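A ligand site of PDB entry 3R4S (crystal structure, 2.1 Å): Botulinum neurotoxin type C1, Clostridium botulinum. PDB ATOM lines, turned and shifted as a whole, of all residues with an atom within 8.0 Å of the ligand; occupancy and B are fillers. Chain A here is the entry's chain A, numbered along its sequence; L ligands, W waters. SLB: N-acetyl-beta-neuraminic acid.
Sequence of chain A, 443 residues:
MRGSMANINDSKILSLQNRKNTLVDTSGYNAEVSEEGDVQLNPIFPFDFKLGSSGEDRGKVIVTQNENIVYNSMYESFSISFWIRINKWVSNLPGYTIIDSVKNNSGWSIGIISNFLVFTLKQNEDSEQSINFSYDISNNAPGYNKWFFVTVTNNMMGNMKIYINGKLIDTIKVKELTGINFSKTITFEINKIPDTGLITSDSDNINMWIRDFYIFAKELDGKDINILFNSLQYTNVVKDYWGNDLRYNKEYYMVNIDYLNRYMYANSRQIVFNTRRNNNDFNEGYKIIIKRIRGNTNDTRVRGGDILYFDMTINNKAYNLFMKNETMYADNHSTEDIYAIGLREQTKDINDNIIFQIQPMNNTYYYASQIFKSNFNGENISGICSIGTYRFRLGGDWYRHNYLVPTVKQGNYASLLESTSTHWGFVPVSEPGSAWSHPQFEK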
ATOM      1  N   MET A 264      35.532  -8.850  26.416  1.00  0.00           N
ATOM      2  CA  MET A 264      34.288  -8.338  25.872  1.00  0.00           C
ATOM      3  C   MET A 264      34.281  -6.811  25.906  1.00  0.00           C
ATOM      4  O   MET A 264      34.572  -6.191  26.941  1.00  0.00           O
ATOM      5  CB  MET A 264      33.120  -8.903  26.670  1.00  0.00           C
ATOM      6  CG  MET A 264      31.860  -9.055  25.881  1.00  0.00           C
ATOM      7  SD  MET A 264      30.577  -9.983  26.744  1.00  0.00           S
ATOM      8  CE  MET A 264      30.711 -11.539  25.868  1.00  0.00           C
ATOM      9  N   TYR A 265      33.983  -6.213  24.766  1.00  0.00           N
ATOM     10  CA  TYR A 265      33.906  -4.760  24.688  1.00  0.00           C
ATOM     11  C   TYR A 265      32.624  -4.367  23.949  1.00  0.00           C
ATOM     12  O   TYR A 265      31.805  -5.221  23.617  1.00  0.00           O
ATOM     13  CB  TYR A 265      35.133  -4.191  23.997  1.00  0.00           C
ATOM     14  CG  TYR A 265      35.340  -2.722  24.256  1.00  0.00           C
ATOM     15  CD1 TYR A 265      35.328  -2.221  25.551  1.00  0.00           C
ATOM     16  CD2 TYR A 265      35.546  -1.837  23.215  1.00  0.00           C
ATOM     17  CE1 TYR A 265      35.514  -0.879  25.803  1.00  0.00           C
ATOM     18  CE2 TYR A 265      35.732  -0.492  23.449  1.00  0.00           C
ATOM     19  CZ  TYR A 265      35.715  -0.014  24.752  1.00  0.00           C
ATOM     20  OH  TYR A 265      35.905   1.338  24.994  1.00  0.00           O
ATOM     21  N   ALA A 266      32.430  -3.072  23.716  1.00  0.00           N
ATOM     22  CA  ALA A 266      31.235  -2.648  22.985  1.00  0.00           C
ATOM     23  C   ALA A 266      31.453  -1.372  22.194  1.00  0.00           C
ATOM     24  O   ALA A 266      32.260  -0.516  22.561  1.00  0.00           O
ATOM     25  CB  ALA A 266      30.035  -2.510  23.922  1.00  0.00           C
ATOM     26  N   ASN A 267      30.706  -1.265  21.113  1.00  0.00           N
ATOM     27  CA  ASN A 267      30.894  -0.205  20.150  1.00  0.00           C
ATOM     28  C   ASN A 267      29.598   0.047  19.396  1.00  0.00           C
ATOM     29  O   ASN A 267      29.171  -0.773  18.590  1.00  0.00           O
ATOM     30  CB  ASN A 267      31.980  -0.627  19.179  1.00  0.00           C
ATOM     31  CG  ASN A 267      32.767   0.529  18.656  1.00  0.00           C
ATOM     32  OD1 ASN A 267      32.217   1.398  17.974  1.00  0.00           O
ATOM     33  ND2 ASN A 267      34.053   0.555  18.983  1.00  0.00           N
ATOM     34  N   SER A 268      28.976   1.183  19.681  1.00  0.00           N
ATOM     35  CA  SER A 268      27.705   1.525  19.081  1.00  0.00           C
ATOM     36  C   SER A 268      26.697   0.452  19.406  1.00  0.00           C
ATOM     37  O   SER A 268      25.898   0.067  18.566  1.00  0.00           O
ATOM     38  CB  SER A 268      27.807   1.670  17.564  1.00  0.00           C
ATOM     39  OG  SER A 268      28.677   2.739  17.211  1.00  0.00           O
ATOM     40  N   ARG A 269      26.742  -0.029  20.643  1.00  0.00           N
ATOM     41  CA  ARG A 269      25.799  -1.017  21.146  1.00  0.00           C
ATOM     42  C   ARG A 269      25.944  -2.394  20.502  1.00  0.00           C
ATOM     43  O   ARG A 269      25.107  -3.279  20.719  1.00  0.00           O
ATOM     44  CB  ARG A 269      24.361  -0.520  20.997  1.00  0.00           C
ATOM     45  CG  ARG A 269      24.027   0.620  21.933  1.00  0.00           C
ATOM     46  CD  ARG A 269      22.605   1.069  21.713  1.00  0.00           C
ATOM     47  NE  ARG A 269      22.226   2.125  22.647  1.00  0.00           N
ATOM     48  CZ  ARG A 269      20.973   2.477  22.890  1.00  0.00           C
ATOM     49  NH1 ARG A 269      19.974   1.845  22.271  1.00  0.00           N
ATOM     50  NH2 ARG A 269      20.711   3.445  23.757  1.00  0.00           N
ATOM     51  N   GLN A 270      27.005  -2.569  19.713  1.00  0.00           N
ATOM     52  CA  GLN A 270      27.374  -3.886  19.230  1.00  0.00           C
ATOM     53  C   GLN A 270      28.512  -4.415  20.101  1.00  0.00           C
ATOM     54  O   GLN A 270      29.559  -3.788  20.214  1.00  0.00           O
ATOM     55  CB  GLN A 270      27.822  -3.836  17.773  1.00  0.00           C
ATOM     56  CG  GLN A 270      28.318  -5.187  17.242  1.00  0.00           C
ATOM     57  CD  GLN A 270      27.317  -6.311  17.518  1.00  0.00           C
ATOM     58  OE1 GLN A 270      27.650  -7.321  18.149  1.00  0.00           O
ATOM     59  NE2 GLN A 270      26.089  -6.115  17.079  1.00  0.00           N
ATOM     60  N   ILE A 271      28.307  -5.573  20.723  1.00  0.00           N
ATOM     61  CA  ILE A 271      29.381  -6.216  21.471  1.00  0.00           C
ATOM     62  C   ILE A 271      30.457  -6.696  20.514  1.00  0.00           C
ATOM     63  O   ILE A 271      30.154  -7.240  19.449  1.00  0.00           O
ATOM     64  CB  ILE A 271      28.888  -7.402  22.308  1.00  0.00           C
ATOM     65  CG1 ILE A 271      27.885  -6.907  23.339  1.00  0.00           C
ATOM     66  CG2 ILE A 271      30.072  -8.102  22.980  1.00  0.00           C
ATOM     67  CD1 ILE A 271      27.221  -8.027  24.122  1.00  0.00           C
ATOM     68  N   VAL A 272      31.713  -6.468  20.889  1.00  0.00           N
ATOM     69  CA  VAL A 272      32.840  -6.909  20.085  1.00  0.00           C
ATOM     70  C   VAL A 272      33.896  -7.504  20.992  1.00  0.00           C
ATOM     71  O   VAL A 272      33.948  -7.198  22.183  1.00  0.00           O
ATOM     72  CB  VAL A 272      33.471  -5.736  19.292  1.00  0.00           C
ATOM     73  CG1 VAL A 272      32.421  -5.068  18.420  1.00  0.00           C
ATOM     74  CG2 VAL A 272      34.088  -4.708  20.239  1.00  0.00           C
ATOM     75  N   TYR A 286      34.190  -5.379  29.696  1.00  0.00           N
ATOM     76  CA  TYR A 286      32.939  -5.287  30.426  1.00  0.00           C
ATOM     77  C   TYR A 286      32.538  -6.620  31.028  1.00  0.00           C
ATOM     78  O   TYR A 286      32.963  -7.694  30.577  1.00  0.00           O
ATOM     79  CB  TYR A 286      31.822  -4.749  29.533  1.00  0.00           C
ATOM     80  CG  TYR A 286      32.125  -3.398  28.931  1.00  0.00           C
ATOM     81  CD1 TYR A 286      32.608  -2.354  29.714  1.00  0.00           C
ATOM     82  CD2 TYR A 286      31.909  -3.150  27.578  1.00  0.00           C
ATOM     83  CE1 TYR A 286      32.876  -1.102  29.161  1.00  0.00           C
ATOM     84  CE2 TYR A 286      32.165  -1.918  27.021  1.00  0.00           C
ATOM     85  CZ  TYR A 286      32.659  -0.898  27.818  1.00  0.00           C
ATOM     86  OH  TYR A 286      32.918   0.340  27.269  1.00  0.00           O
ATOM     87  N   MET A 312      24.443  -5.941  31.019  1.00  0.00           N
ATOM     88  CA  MET A 312      25.774  -5.353  30.976  1.00  0.00           C
ATOM     89  C   MET A 312      25.692  -3.839  31.258  1.00  0.00           C
ATOM     90  O   MET A 312      24.866  -3.126  30.691  1.00  0.00           O
ATOM     91  CB  MET A 312      26.423  -5.605  29.615  1.00  0.00           C
ATOM     92  CG  MET A 312      27.815  -4.992  29.484  1.00  0.00           C
ATOM     93  SD  MET A 312      28.534  -5.279  27.863  1.00  0.00           S
ATOM     94  CE  MET A 312      28.870  -7.048  27.925  1.00  0.00           C
ATOM     95  N   THR A 313      26.531  -3.359  32.165  1.00  0.00           N
ATOM     96  CA  THR A 313      26.533  -1.941  32.493  1.00  0.00           C
ATOM     97  C   THR A 313      27.751  -1.249  31.890  1.00  0.00           C
ATOM     98  O   THR A 313      28.893  -1.677  32.088  1.00  0.00           O
ATOM     99  CB  THR A 313      26.501  -1.711  34.021  1.00  0.00           C
ATOM    100  OG1 THR A 313      25.216  -2.113  34.531  1.00  0.00           O
ATOM    101  CG2 THR A 313      26.718  -0.245  34.351  1.00  0.00           C
ATOM    102  N   ILE A 314      27.497  -0.194  31.129  1.00  0.00           N
ATOM    103  CA  ILE A 314      28.564   0.615  30.545  1.00  0.00           C
ATOM    104  C   ILE A 314      28.300   2.089  30.856  1.00  0.00           C
ATOM    105  O   ILE A 314      27.191   2.582  30.640  1.00  0.00           O
ATOM    106  CB  ILE A 314      28.640   0.438  29.032  1.00  0.00           C
ATOM    107  CG1 ILE A 314      28.852  -1.035  28.679  1.00  0.00           C
ATOM    108  CG2 ILE A 314      29.739   1.310  28.446  1.00  0.00           C
ATOM    109  CD1 ILE A 314      28.766  -1.325  27.202  1.00  0.00           C
ATOM    110  N   ASN A 315      29.321   2.779  31.368  1.00  0.00           N
ATOM    111  CA  ASN A 315      29.192   4.199  31.716  1.00  0.00           C
ATOM    112  C   ASN A 315      27.935   4.459  32.523  1.00  0.00           C
ATOM    113  O   ASN A 315      27.173   5.392  32.237  1.00  0.00           O
ATOM    114  CB  ASN A 315      29.227   5.074  30.451  1.00  0.00           C
ATOM    115  CG  ASN A 315      30.556   4.973  29.710  1.00  0.00           C
ATOM    116  OD1 ASN A 315      30.597   5.070  28.476  1.00  0.00           O
ATOM    117  ND2 ASN A 315      31.638   4.767  30.453  1.00  0.00           N
ATOM    118  N   LYS A 317      25.111   3.123  32.568  1.00  0.00           N
ATOM    119  CA  LYS A 317      23.834   2.781  31.954  1.00  0.00           C
ATOM    120  C   LYS A 317      23.748   1.261  31.854  1.00  0.00           C
ATOM    121  O   LYS A 317      24.717   0.610  31.447  1.00  0.00           O
ATOM    122  CB  LYS A 317      23.730   3.395  30.565  1.00  0.00           C
ATOM    123  CG  LYS A 317      22.463   3.015  29.817  1.00  0.00           C
ATOM    124  CD  LYS A 317      21.392   4.094  29.929  1.00  0.00           C
ATOM    125  CE  LYS A 317      21.768   5.331  29.120  1.00  0.00           C
ATOM    126  NZ  LYS A 317      21.736   5.045  27.651  1.00  0.00           N
ATOM    127  N   TYR A 319      22.303  -2.180  30.243  1.00  0.00           N
ATOM    128  CA  TYR A 319      21.708  -2.749  29.043  1.00  0.00           C
ATOM    129  C   TYR A 319      21.331  -4.226  29.215  1.00  0.00           C
ATOM    130  O   TYR A 319      21.722  -4.873  30.181  1.00  0.00           O
ATOM    131  CB  TYR A 319      22.690  -2.666  27.887  1.00  0.00           C
ATOM    132  CG  TYR A 319      23.181  -1.269  27.554  1.00  0.00           C
ATOM    133  CD1 TYR A 319      22.575  -0.509  26.563  1.00  0.00           C
ATOM    134  CD2 TYR A 319      24.274  -0.720  28.217  1.00  0.00           C
ATOM    135  CE1 TYR A 319      23.032   0.766  26.241  1.00  0.00           C
ATOM    136  CE2 TYR A 319      24.742   0.545  27.911  1.00  0.00           C
ATOM    137  CZ  TYR A 319      24.115   1.284  26.922  1.00  0.00           C
ATOM    138  OH  TYR A 319      24.579   2.543  26.609  1.00  0.00           O
ATOM    139  N   LEU A 343      23.489  -4.791  22.368  1.00  0.00           N
ATOM    140  CA  LEU A 343      22.998  -4.251  23.631  1.00  0.00           C
ATOM    141  C   LEU A 343      21.853  -3.271  23.422  1.00  0.00           C
ATOM    142  O   LEU A 343      21.924  -2.393  22.556  1.00  0.00           O
ATOM    143  CB  LEU A 343      24.130  -3.586  24.417  1.00  0.00           C
ATOM    144  CG  LEU A 343      25.360  -4.451  24.692  1.00  0.00           C
ATOM    145  CD1 LEU A 343      26.587  -3.581  24.951  1.00  0.00           C
ATOM    146  CD2 LEU A 343      25.104  -5.390  25.871  1.00  0.00           C
ATOM    147  N   ARG A 344      20.811  -3.413  24.228  1.00  0.00           N
ATOM    148  CA  ARG A 344      19.662  -2.520  24.170  1.00  0.00           C
ATOM    149  C   ARG A 344      19.296  -2.051  25.578  1.00  0.00           C
ATOM    150  O   ARG A 344      19.503  -2.766  26.569  1.00  0.00           O
ATOM    151  CB  ARG A 344      18.465  -3.213  23.535  1.00  0.00           C
ATOM    152  CG  ARG A 344      17.972  -4.407  24.336  1.00  0.00           C
ATOM    153  CD  ARG A 344      16.656  -4.940  23.809  1.00  0.00           C
ATOM    154  NE  ARG A 344      15.580  -3.968  23.974  1.00  0.00           N
ATOM    155  CZ  ARG A 344      14.310  -4.194  23.635  1.00  0.00           C
ATOM    156  NH1 ARG A 344      13.963  -5.369  23.117  1.00  0.00           N
ATOM    157  NH2 ARG A 344      13.395  -3.261  23.823  1.00  0.00           N
ATOM    158  N   LEU A 394      30.704   0.682  12.807  1.00  0.00           N
ATOM    159  CA  LEU A 394      30.523   1.075  14.198  1.00  0.00           C
ATOM    160  C   LEU A 394      31.335   2.318  14.517  1.00  0.00           C
ATOM    161  O   LEU A 394      32.335   2.590  13.857  1.00  0.00           O
ATOM    162  CB  LEU A 394      30.949  -0.068  15.120  1.00  0.00           C
ATOM    163  CG  LEU A 394      30.389  -1.476  14.877  1.00  0.00           C
ATOM    164  CD1 LEU A 394      31.071  -2.493  15.797  1.00  0.00           C
ATOM    165  CD2 LEU A 394      28.876  -1.490  15.058  1.00  0.00           C
ATOM    166  N   GLY A 395      30.909   3.066  15.515  1.00  0.00           N
ATOM    167  CA  GLY A 395      31.687   4.181  16.025  1.00  0.00           C
ATOM    168  C   GLY A 395      32.204   5.185  15.010  1.00  0.00           C
ATOM    169  O   GLY A 395      33.385   5.555  15.030  1.00  0.00           O
ATOM    170  N   GLY A 396      31.341   5.634  14.112  1.00  0.00           N
ATOM    171  CA  GLY A 396      31.752   6.660  13.173  1.00  0.00           C
ATOM    172  C   GLY A 396      32.381   6.171  11.869  1.00  0.00           C
ATOM    173  O   GLY A 396      32.524   6.959  10.922  1.00  0.00           O
HETATM  174  C1  SLB L   1      34.292   4.531  23.278  1.00  0.00           C
HETATM  175  C2  SLB L   1      32.973   4.144  23.883  1.00  0.00           C
HETATM  176  C3  SLB L   1      33.009   2.651  24.240  1.00  0.00           C
HETATM  177  C4  SLB L   1      31.652   2.174  24.742  1.00  0.00           C
HETATM  178  C5  SLB L   1      30.613   2.441  23.671  1.00  0.00           C
HETATM  179  C6  SLB L   1      30.610   3.932  23.326  1.00  0.00           C
HETATM  180  C7  SLB L   1      29.665   4.146  22.157  1.00  0.00           C
HETATM  181  C8  SLB L   1      29.406   5.645  21.916  1.00  0.00           C
HETATM  182  C9  SLB L   1      28.421   5.871  20.777  1.00  0.00           C
HETATM  183  C10 SLB L   1      28.394   1.409  23.767  1.00  0.00           C
HETATM  184  C11 SLB L   1      27.140   1.289  24.583  1.00  0.00           C
HETATM  185  N5  SLB L   1      29.328   2.185  24.302  1.00  0.00           N
HETATM  186  O1A SLB L   1      34.558   4.211  22.094  1.00  0.00           O
HETATM  187  O1B SLB L   1      35.100   5.154  24.008  1.00  0.00           O
HETATM  188  O2  SLB L   1      32.813   4.908  25.084  1.00  0.00           O
HETATM  189  O4  SLB L   1      31.685   0.765  25.012  1.00  0.00           O
HETATM  190  O6  SLB L   1      31.908   4.446  22.974  1.00  0.00           O
HETATM  191  O7  SLB L   1      30.306   3.541  21.005  1.00  0.00           O
HETATM  192  O8  SLB L   1      28.895   6.252  23.119  1.00  0.00           O
HETATM  193  O9  SLB L   1      29.142   5.827  19.541  1.00  0.00           O
HETATM  194  O10 SLB L   1      28.539   0.819  22.703  1.00  0.00           O
HETATM  195  O   HOH W   1      26.140   6.310  23.969  1.00  0.00           O
HETATM  196  O   HOH W   2      28.493   4.192  26.514  1.00  0.00           O
HETATM  197  O   HOH W   3      25.869   3.882  21.573  1.00  0.00           O
HETATM  198  O   HOH W   4      32.679   3.811  19.842  1.00  0.00           O
HETATM  199  O   HOH W   5      29.808   7.106  17.363  1.00  0.00           O
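The backbone NH (N) of Leu 343 sits at hydrogen-bond distance from the backbone carbonyl oxygen (O) of Arg 269, 2.8 Å away.
The backbone NH of Gly 395 lies within hydrogen-bond range of the side-chain amide oxygen of Asn 267 (3.2 Å).
The backbone NH (N) of Tyr 319 sits at hydrogen-bond distance from the backbone carbonyl oxygen (O) of Met 312, at 2.8 Å.
The side-chain hydroxyl of Ser 268 lies within hydrogen-bond range of the backbone NH of Gly 395 (2.8 Å).
The backbone carbonyl oxygen (O) of Val 272 is in hydrogen-bond range of the backbone NH (N) of Tyr 265 (2.8 Å).
The backbone NH (N) of Tyr 286 sits at hydrogen-bond distance from the backbone carbonyl oxygen (O) of Met 264, at 2.9 Å.
An oxygen (O4) of the ligand is in hydrogen-bond range of the side-chain hydroxyl (OH) of Tyr 286.
The backbone NH (N) of Asn 267 lies within hydrogen-bond range of an oxygen (O10) of the ligand.
N of Ser 268 lies within hydrogen-bond range of O7 of the ligand, 3.0 Å away.
O4 of the ligand lies within hydrogen-bond range of O of Ala 266 (2.8 Å).
O10 of the ligand is in hydrogen-bond range of N of Arg 269.
Merely in contact with the ligand: Tyr 265 (3.3 Å), Tyr 319 (3.5 Å) and Ile 314 (3.98 Å).
Hydrophobic or aromatic side chains within 4 Å of the ligand: Tyr 265, Ala 266, Tyr 286, Ile 314 and Tyr 319.
Of the 21 residues printed, 8 come within 4 Å of the ligand.
Water W4 bridges O7 of the ligand and OD1 of Asn 267.
Water W2 bridges the side-chain amide oxygen of Asn 315 and a nitrogen (N5) of the ligand.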
